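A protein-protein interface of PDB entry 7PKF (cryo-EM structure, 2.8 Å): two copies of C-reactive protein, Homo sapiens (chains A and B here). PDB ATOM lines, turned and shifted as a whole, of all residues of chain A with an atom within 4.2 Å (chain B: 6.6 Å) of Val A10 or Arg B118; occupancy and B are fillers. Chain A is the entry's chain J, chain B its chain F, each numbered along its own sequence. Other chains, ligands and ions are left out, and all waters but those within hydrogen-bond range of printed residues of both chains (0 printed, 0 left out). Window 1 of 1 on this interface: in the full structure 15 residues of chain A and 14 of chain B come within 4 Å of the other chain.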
ATOM      1  N   ALA A   8       9.034  -8.743  30.446  1.00  0.00           N
ATOM      2  CA  ALA A   8       9.433  -9.108  29.097  1.00  0.00           C
ATOM      3  C   ALA A   8      10.876  -8.693  28.852  1.00  0.00           C
ATOM      4  O   ALA A   8      11.374  -7.735  29.445  1.00  0.00           O
ATOM      5  CB  ALA A   8       8.523  -8.458  28.051  1.00  0.00           C
ATOM      6  N   PHE A   9      11.541  -9.434  27.971  1.00  0.00           N
ATOM      7  CA  PHE A   9      12.809  -8.999  27.404  1.00  0.00           C
ATOM      8  C   PHE A   9      12.551  -8.022  26.266  1.00  0.00           C
ATOM      9  O   PHE A   9      11.720  -8.282  25.391  1.00  0.00           O
ATOM     10  CB  PHE A   9      13.612 -10.200  26.912  1.00  0.00           C
ATOM     11  CG  PHE A   9      14.066 -11.111  28.013  1.00  0.00           C
ATOM     12  CD1 PHE A   9      14.896 -10.645  29.014  1.00  0.00           C
ATOM     13  CD2 PHE A   9      13.672 -12.432  28.041  1.00  0.00           C
ATOM     14  CE1 PHE A   9      15.321 -11.480  30.023  1.00  0.00           C
ATOM     15  CE2 PHE A   9      14.094 -13.271  29.048  1.00  0.00           C
ATOM     16  CZ  PHE A   9      14.918 -12.793  30.040  1.00  0.00           C
ATOM     17  N   VAL A  10      13.265  -6.900  26.277  1.00  0.00           N
ATOM     18  CA  VAL A  10      13.108  -5.852  25.277  1.00  0.00           C
ATOM     19  C   VAL A  10      14.369  -5.800  24.428  1.00  0.00           C
ATOM     20  O   VAL A  10      15.479  -5.670  24.958  1.00  0.00           O
ATOM     21  CB  VAL A  10      12.847  -4.486  25.937  1.00  0.00           C
ATOM     22  CG1 VAL A  10      12.421  -3.461  24.899  1.00  0.00           C
ATOM     23  CG2 VAL A  10      11.820  -4.611  27.049  1.00  0.00           C
ATOM     24  N   PHE A  11      14.195  -5.902  23.114  1.00  0.00           N
ATOM     25  CA  PHE A  11      15.288  -5.796  22.159  1.00  0.00           C
ATOM     26  C   PHE A  11      15.086  -4.549  21.310  1.00  0.00           C
ATOM     27  O   PHE A  11      14.548  -4.644  20.202  1.00  0.00           O
ATOM     28  CB  PHE A  11      15.351  -7.033  21.265  1.00  0.00           C
ATOM     29  CG  PHE A  11      15.600  -8.308  22.009  1.00  0.00           C
ATOM     30  CD1 PHE A  11      16.873  -8.832  22.106  1.00  0.00           C
ATOM     31  CD2 PHE A  11      14.550  -9.007  22.572  1.00  0.00           C
ATOM     32  CE1 PHE A  11      17.096 -10.014  22.777  1.00  0.00           C
ATOM     33  CE2 PHE A  11      14.768 -10.186  23.245  1.00  0.00           C
ATOM     34  CZ  PHE A  11      16.043 -10.687  23.353  1.00  0.00           C
ATOM     35  N   PRO A  12      15.485  -3.370  21.783  1.00  0.00           N
ATOM     36  CA  PRO A  12      15.015  -2.124  21.165  1.00  0.00           C
ATOM     37  C   PRO A  12      15.822  -1.645  19.967  1.00  0.00           C
ATOM     38  O   PRO A  12      15.504  -0.581  19.424  1.00  0.00           O
ATOM     39  CB  PRO A  12      15.136  -1.140  22.331  1.00  0.00           C
ATOM     40  CG  PRO A  12      16.363  -1.594  23.022  1.00  0.00           C
ATOM     41  CD  PRO A  12      16.275  -3.100  22.996  1.00  0.00           C
ATOM     42  N   GLY A 154      11.874  -5.509  19.430  1.00  0.00           N
ATOM     43  CA  GLY A 154      10.637  -5.483  20.184  1.00  0.00           C
ATOM     44  C   GLY A 154      10.710  -6.376  21.412  1.00  0.00           C
ATOM     45  O   GLY A 154      11.778  -6.546  22.013  1.00  0.00           O
ATOM     46  N   ASP A 155       9.563  -6.948  21.775  1.00  0.00           N
ATOM     47  CA  ASP A 155       9.397  -7.609  23.061  1.00  0.00           C
ATOM     48  C   ASP A 155       9.090  -9.086  22.868  1.00  0.00           C
ATOM     49  O   ASP A 155       8.428  -9.476  21.904  1.00  0.00           O
ATOM     50  CB  ASP A 155       8.260  -6.964  23.858  1.00  0.00           C
ATOM     51  CG  ASP A 155       8.584  -5.558  24.302  1.00  0.00           C
ATOM     52  OD1 ASP A 155       9.472  -5.397  25.158  1.00  0.00           O
ATOM     53  OD2 ASP A 155       7.950  -4.610  23.795  1.00  0.00           O
ATOM     54  N   VAL A 198      20.037  -5.853  25.957  1.00  0.00           N
ATOM     55  CA  VAL A 198      18.710  -6.401  26.203  1.00  0.00           C
ATOM     56  C   VAL A 198      18.249  -5.932  27.573  1.00  0.00           C
ATOM     57  O   VAL A 198      19.028  -5.933  28.533  1.00  0.00           O
ATOM     58  CB  VAL A 198      18.694  -7.941  26.126  1.00  0.00           C
ATOM     59  CG1 VAL A 198      17.277  -8.465  26.271  1.00  0.00           C
ATOM     60  CG2 VAL A 198      19.302  -8.415  24.821  1.00  0.00           C
ATOM     61  N   PHE A 199      16.985  -5.533  27.665  1.00  0.00           N
ATOM     62  CA  PHE A 199      16.422  -5.002  28.894  1.00  0.00           C
ATOM     63  C   PHE A 199      15.233  -5.842  29.337  1.00  0.00           C
ATOM     64  O   PHE A 199      14.531  -6.440  28.518  1.00  0.00           O
ATOM     65  CB  PHE A 199      15.998  -3.545  28.707  1.00  0.00           C
ATOM     66  CG  PHE A 199      17.111  -2.656  28.240  1.00  0.00           C
ATOM     67  CD1 PHE A 199      17.278  -2.388  26.894  1.00  0.00           C
ATOM     68  CD2 PHE A 199      18.003  -2.109  29.142  1.00  0.00           C
ATOM     69  CE1 PHE A 199      18.304  -1.577  26.460  1.00  0.00           C
ATOM     70  CE2 PHE A 199      19.031  -1.297  28.712  1.00  0.00           C
ATOM     71  CZ  PHE A 199      19.182  -1.033  27.368  1.00  0.00           C
ATOM     72  N   LYS A 201      11.676  -5.328  31.158  1.00  0.00           N
ATOM     73  CA  LYS A 201      10.708  -4.286  31.457  1.00  0.00           C
ATOM     74  C   LYS A 201       9.357  -4.929  31.724  1.00  0.00           C
ATOM     75  O   LYS A 201       9.128  -6.082  31.347  1.00  0.00           O
ATOM     76  CB  LYS A 201      10.589  -3.285  30.299  1.00  0.00           C
ATOM     77  CG  LYS A 201      11.810  -2.410  30.083  1.00  0.00           C
ATOM     78  CD  LYS A 201      12.107  -1.542  31.290  1.00  0.00           C
ATOM     79  CE  LYS A 201      13.232  -0.566  31.005  1.00  0.00           C
ATOM     80  NZ  LYS A 201      13.690   0.124  32.238  1.00  0.00           N
ATOM     81  N   PRO A 202       8.445  -4.211  32.377  1.00  0.00           N
ATOM     82  CA  PRO A 202       7.058  -4.684  32.471  1.00  0.00           C
ATOM     83  C   PRO A 202       6.453  -4.997  31.111  1.00  0.00           C
ATOM     84  O   PRO A 202       6.545  -4.207  30.171  1.00  0.00           O
ATOM     85  CB  PRO A 202       6.334  -3.523  33.161  1.00  0.00           C
ATOM     86  CG  PRO A 202       7.398  -2.732  33.823  1.00  0.00           C
ATOM     87  CD  PRO A 202       8.611  -2.876  32.974  1.00  0.00           C
ATOM     88  N   GLN A 203       5.828  -6.168  31.010  1.00  0.00           N
ATOM     89  CA  GLN A 203       5.189  -6.575  29.766  1.00  0.00           C
ATOM     90  C   GLN A 203       4.094  -5.588  29.369  1.00  0.00           C
ATOM     91  O   GLN A 203       3.328  -5.114  30.211  1.00  0.00           O
ATOM     92  CB  GLN A 203       4.628  -7.989  29.910  1.00  0.00           C
ATOM     93  CG  GLN A 203       3.422  -8.102  30.815  1.00  0.00           C
ATOM     94  CD  GLN A 203       2.896  -9.515  30.899  1.00  0.00           C
ATOM     95  OE1 GLN A 203       3.661 -10.462  31.061  1.00  0.00           O
ATOM     96  NE2 GLN A 203       1.585  -9.667  30.784  1.00  0.00           N
ATOM     97  N   LEU A 204       4.030  -5.272  28.073  1.00  0.00           N
ATOM     98  CA  LEU A 204       3.023  -4.341  27.569  1.00  0.00           C
ATOM     99  C   LEU A 204       1.641  -4.979  27.487  1.00  0.00           C
ATOM    100  O   LEU A 204       0.629  -4.307  27.712  1.00  0.00           O
ATOM    101  CB  LEU A 204       3.429  -3.816  26.192  1.00  0.00           C
ATOM    102  CG  LEU A 204       4.712  -2.992  26.114  1.00  0.00           C
ATOM    103  CD1 LEU A 204       5.128  -2.792  24.670  1.00  0.00           C
ATOM    104  CD2 LEU A 204       4.529  -1.659  26.808  1.00  0.00           C
ATOM    105  N   PHE B  84       6.605   6.507  14.833  1.00  0.00           N
ATOM    106  CA  PHE B  84       5.529   5.534  15.059  1.00  0.00           C
ATOM    107  C   PHE B  84       4.464   5.663  13.980  1.00  0.00           C
ATOM    108  O   PHE B  84       3.488   6.399  14.132  1.00  0.00           O
ATOM    109  CB  PHE B  84       5.024   5.707  16.468  1.00  0.00           C
ATOM    110  CG  PHE B  84       6.100   5.506  17.468  1.00  0.00           C
ATOM    111  CD1 PHE B  84       6.409   4.230  17.891  1.00  0.00           C
ATOM    112  CD2 PHE B  84       6.913   6.542  17.861  1.00  0.00           C
ATOM    113  CE1 PHE B  84       7.422   4.010  18.768  1.00  0.00           C
ATOM    114  CE2 PHE B  84       7.952   6.318  18.717  1.00  0.00           C
ATOM    115  CZ  PHE B  84       8.210   5.048  19.171  1.00  0.00           C
ATOM    116  N   ILE B 106      14.757   3.632  26.295  1.00  0.00           N
ATOM    117  CA  ILE B 106      13.504   3.096  25.775  1.00  0.00           C
ATOM    118  C   ILE B 106      12.464   4.209  25.737  1.00  0.00           C
ATOM    119  O   ILE B 106      12.247   4.910  26.733  1.00  0.00           O
ATOM    120  CB  ILE B 106      13.046   1.892  26.610  1.00  0.00           C
ATOM    121  CG1 ILE B 106      14.053   0.751  26.452  1.00  0.00           C
ATOM    122  CG2 ILE B 106      11.676   1.422  26.166  1.00  0.00           C
ATOM    123  CD1 ILE B 106      13.917  -0.329  27.480  1.00  0.00           C
ATOM    124  N   VAL B 107      11.818   4.381  24.588  1.00  0.00           N
ATOM    125  CA  VAL B 107      10.616   5.200  24.459  1.00  0.00           C
ATOM    126  C   VAL B 107       9.391   4.282  24.415  1.00  0.00           C
ATOM    127  O   VAL B 107       9.325   3.366  23.587  1.00  0.00           O
ATOM    128  CB  VAL B 107      10.710   6.115  23.231  1.00  0.00           C
ATOM    129  CG1 VAL B 107       9.488   6.962  23.126  1.00  0.00           C
ATOM    130  CG2 VAL B 107      11.950   6.998  23.325  1.00  0.00           C
ATOM    131  N   GLU B 108       8.425   4.522  25.310  1.00  0.00           N
ATOM    132  CA  GLU B 108       7.082   3.934  25.257  1.00  0.00           C
ATOM    133  C   GLU B 108       5.994   4.884  24.749  1.00  0.00           C
ATOM    134  O   GLU B 108       5.836   5.988  25.272  1.00  0.00           O
ATOM    135  CB  GLU B 108       6.687   3.427  26.644  1.00  0.00           C
ATOM    136  CG  GLU B 108       7.435   2.195  27.087  1.00  0.00           C
ATOM    137  CD  GLU B 108       6.974   1.682  28.436  1.00  0.00           C
ATOM    138  OE1 GLU B 108       5.812   1.941  28.810  1.00  0.00           O
ATOM    139  OE2 GLU B 108       7.778   1.015  29.122  1.00  0.00           O
ATOM    140  N   PHE B 109       5.277   4.448  23.712  1.00  0.00           N
ATOM    141  CA  PHE B 109       4.070   5.076  23.163  1.00  0.00           C
ATOM    142  C   PHE B 109       2.794   4.277  23.314  1.00  0.00           C
ATOM    143  O   PHE B 109       2.735   3.097  22.958  1.00  0.00           O
ATOM    144  CB  PHE B 109       4.220   5.466  21.705  1.00  0.00           C
ATOM    145  CG  PHE B 109       5.116   6.576  21.527  1.00  0.00           C
ATOM    146  CD1 PHE B 109       4.608   7.836  21.729  1.00  0.00           C
ATOM    147  CD2 PHE B 109       6.440   6.425  21.300  1.00  0.00           C
ATOM    148  CE1 PHE B 109       5.377   8.912  21.606  1.00  0.00           C
ATOM    149  CE2 PHE B 109       7.214   7.524  21.188  1.00  0.00           C
ATOM    150  CZ  PHE B 109       6.675   8.754  21.365  1.00  0.00           C
ATOM    151  N   ARG B 116       2.352   1.114  21.544  1.00  0.00           N
ATOM    152  CA  ARG B 116       3.301   0.814  20.484  1.00  0.00           C
ATOM    153  C   ARG B 116       4.475  -0.017  21.006  1.00  0.00           C
ATOM    154  O   ARG B 116       4.730  -0.102  22.210  1.00  0.00           O
ATOM    155  CB  ARG B 116       3.803   2.097  19.827  1.00  0.00           C
ATOM    156  CG  ARG B 116       2.692   3.020  19.350  1.00  0.00           C
ATOM    157  CD  ARG B 116       1.836   2.356  18.281  1.00  0.00           C
ATOM    158  NE  ARG B 116       2.584   2.160  17.041  1.00  0.00           N
ATOM    159  CZ  ARG B 116       2.417   2.854  15.921  1.00  0.00           C
ATOM    160  NH1 ARG B 116       1.379   3.665  15.765  1.00  0.00           N
ATOM    161  NH2 ARG B 116       3.201   2.602  14.882  1.00  0.00           N
ATOM    162  N   VAL B 117       5.196  -0.635  20.066  1.00  0.00           N
ATOM    163  CA  VAL B 117       6.463  -1.293  20.379  1.00  0.00           C
ATOM    164  C   VAL B 117       7.458  -0.311  20.993  1.00  0.00           C
ATOM    165  O   VAL B 117       7.628   0.819  20.520  1.00  0.00           O
ATOM    166  CB  VAL B 117       7.037  -1.942  19.107  1.00  0.00           C
ATOM    167  CG1 VAL B 117       8.416  -2.527  19.367  1.00  0.00           C
ATOM    168  CG2 VAL B 117       6.097  -3.016  18.587  1.00  0.00           C
ATOM    169  N   ARG B 118       8.120  -0.754  22.061  1.00  0.00           N
ATOM    170  CA  ARG B 118       9.223  -0.013  22.674  1.00  0.00           C
ATOM    171  C   ARG B 118      10.417   0.152  21.739  1.00  0.00           C
ATOM    172  O   ARG B 118      10.983  -0.834  21.258  1.00  0.00           O
ATOM    173  CB  ARG B 118       9.669  -0.680  23.974  1.00  0.00           C
ATOM    174  CG  ARG B 118       8.803  -0.313  25.162  1.00  0.00           C
ATOM    175  CD  ARG B 118       9.186  -1.051  26.434  1.00  0.00           C
ATOM    176  NE  ARG B 118       8.600  -2.381  26.556  1.00  0.00           N
ATOM    177  CZ  ARG B 118       8.028  -2.863  27.659  1.00  0.00           C
ATOM    178  NH1 ARG B 118       7.810  -2.090  28.716  1.00  0.00           N
ATOM    179  NH2 ARG B 118       7.538  -4.092  27.646  1.00  0.00           N
ATOM    180  N   LYS B 119      10.792   1.402  21.480  1.00  0.00           N
ATOM    181  CA  LYS B 119      11.927   1.764  20.643  1.00  0.00           C
ATOM    182  C   LYS B 119      13.003   2.403  21.520  1.00  0.00           C
ATOM    183  O   LYS B 119      12.762   2.741  22.679  1.00  0.00           O
ATOM    184  CB  LYS B 119      11.488   2.703  19.516  1.00  0.00           C
ATOM    185  CG  LYS B 119      10.423   2.083  18.625  1.00  0.00           C
ATOM    186  CD  LYS B 119      10.237   2.823  17.316  1.00  0.00           C
ATOM    187  CE  LYS B 119       9.198   2.124  16.451  1.00  0.00           C
ATOM    188  NZ  LYS B 119       9.151   2.655  15.065  1.00  0.00           N
ATOM    189  N   SER B 120      14.200   2.574  20.960  1.00  0.00           N
ATOM    190  CA  SER B 120      15.318   3.206  21.656  1.00  0.00           C
ATOM    191  C   SER B 120      15.604   4.607  21.136  1.00  0.00           C
ATOM    192  O   SER B 120      15.620   4.843  19.925  1.00  0.00           O
ATOM    193  CB  SER B 120      16.587   2.363  21.515  1.00  0.00           C
ATOM    194  OG  SER B 120      17.627   2.866  22.331  1.00  0.00           O
ATOM    195  N   PRO B 168       2.913   0.183  32.632  1.00  0.00           N
ATOM    196  CA  PRO B 168       1.634  -0.084  31.940  1.00  0.00           C
ATOM    197  C   PRO B 168       0.379  -0.087  32.804  1.00  0.00           C
ATOM    198  O   PRO B 168      -0.661   0.398  32.346  1.00  0.00           O
ATOM    199  CB  PRO B 168       1.871  -1.465  31.313  1.00  0.00           C
ATOM    200  CG  PRO B 168       3.339  -1.578  31.176  1.00  0.00           C
ATOM    201  CD  PRO B 168       3.920  -0.850  32.341  1.00  0.00           C
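OD1 of Asp A155 lies within salt-bridge range of NH2 of Arg B118.
The backbone carbonyl oxygen (O) of Pro A202 sits at hydrogen-bond distance from the guanidinium group (NH2) of Arg B118.
Printed residues of chain B that touch a printed residue of chain A: Ile B106, Arg B116, Val B117, Arg B118, Ser B120 and Pro B168.
Hydrophobic or aromatic side chains of chain B that line the printed part of chain A: Ile B106, Val B117 and Pro B168.
Along chain B the printed residues that touch a printed residue of chain A span positions 106 to 168.
Of the 13 printed residues of chain A, 9 touch a printed residue of chain B.
Printed residues of chain A that touch a printed residue of chain B: Val A10, Pro A12, Gly A154, Asp A155, Phe A199, Lys A201, Pro A202, Gln A203 and Leu A204.
Hydrophobic or aromatic side chains of chain A that line the printed part of chain B: Val A10, Pro A12, Phe A199, Pro A202 and Leu A204.
Among the printed residues, 12 pairs touch across the chains.
Among the printed residues, Asp or Glu carboxylates within 4 Å of a Lys or Arg side-chain nitrogen of the other chain: Asp A155 with Arg B118 (3.4 Å).
The side-chain carboxylate of Glu B108 lies within salt-bridge range of the guanidinium group of Arg B118, 3.1 Å away.
O of Phe B109 sits at hydrogen-bond distance from N of Arg B116 (2.5 Å).
The backbone NH (N) of Phe A11 is in hydrogen-bond range of the backbone carbonyl oxygen (O) of Gly A154, at 2.7 Å.
N of Val A10 is in hydrogen-bond range of O of Phe A199 (2.6 Å).
The backbone carbonyl oxygen (O) of Lys A201 sits at hydrogen-bond distance from the backbone NH (N) of Ala A8.
No position is printed for both chains.
Of the 12 pairs that touch across the chains among the printed residues, none has its exchanged pair printed and touching as well.
NE of Arg B118 touches CG2 of Val A10, at 3.9 Å.
N of Ser B120 touches O of Pro A12, 3.7 Å away.
CG1 of Val B117 touches CA of Gly A154, at 3.8 Å.
Phe A199 touches Ile B106.
Lys A201 touches Ile B106.
Lys A201 touches Arg B118 (CB to NH1, 3.4 Å).
Pro B168 touches Pro A202 (CD to CB, 3.7 Å).
Gln A203 touches Pro B168.
Leu A204 touches Arg B116 (CD1 to O, 3.7 Å).
NH2 of Arg B118 touches CG of Leu A204, 3.4 Å away.
Val A10 touches just one residue of chain B: Arg B118 (3.9 Å).
Of chain A, only Val A10 (3.9 Å), Asp A155 (3.4 Å), Lys A201 (3.4 Å), Pro A202 (2.7 Å) and Leu A204 (3.4 Å) come within 4 Å of Arg B118.
Of the printed residues of chain B, Leu A204 touches Arg B116 and Arg B118.
Of the printed residues of chain B, Phe A199 touches Ile B106 (3.98 Å).
Of the printed residues of chain B, Gln A203 touches Pro B168.
Of the printed residues of chain A, Val B117 touches Gly A154 (3.8 Å).
Phe B84 touches none of the printed residues of chain A.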
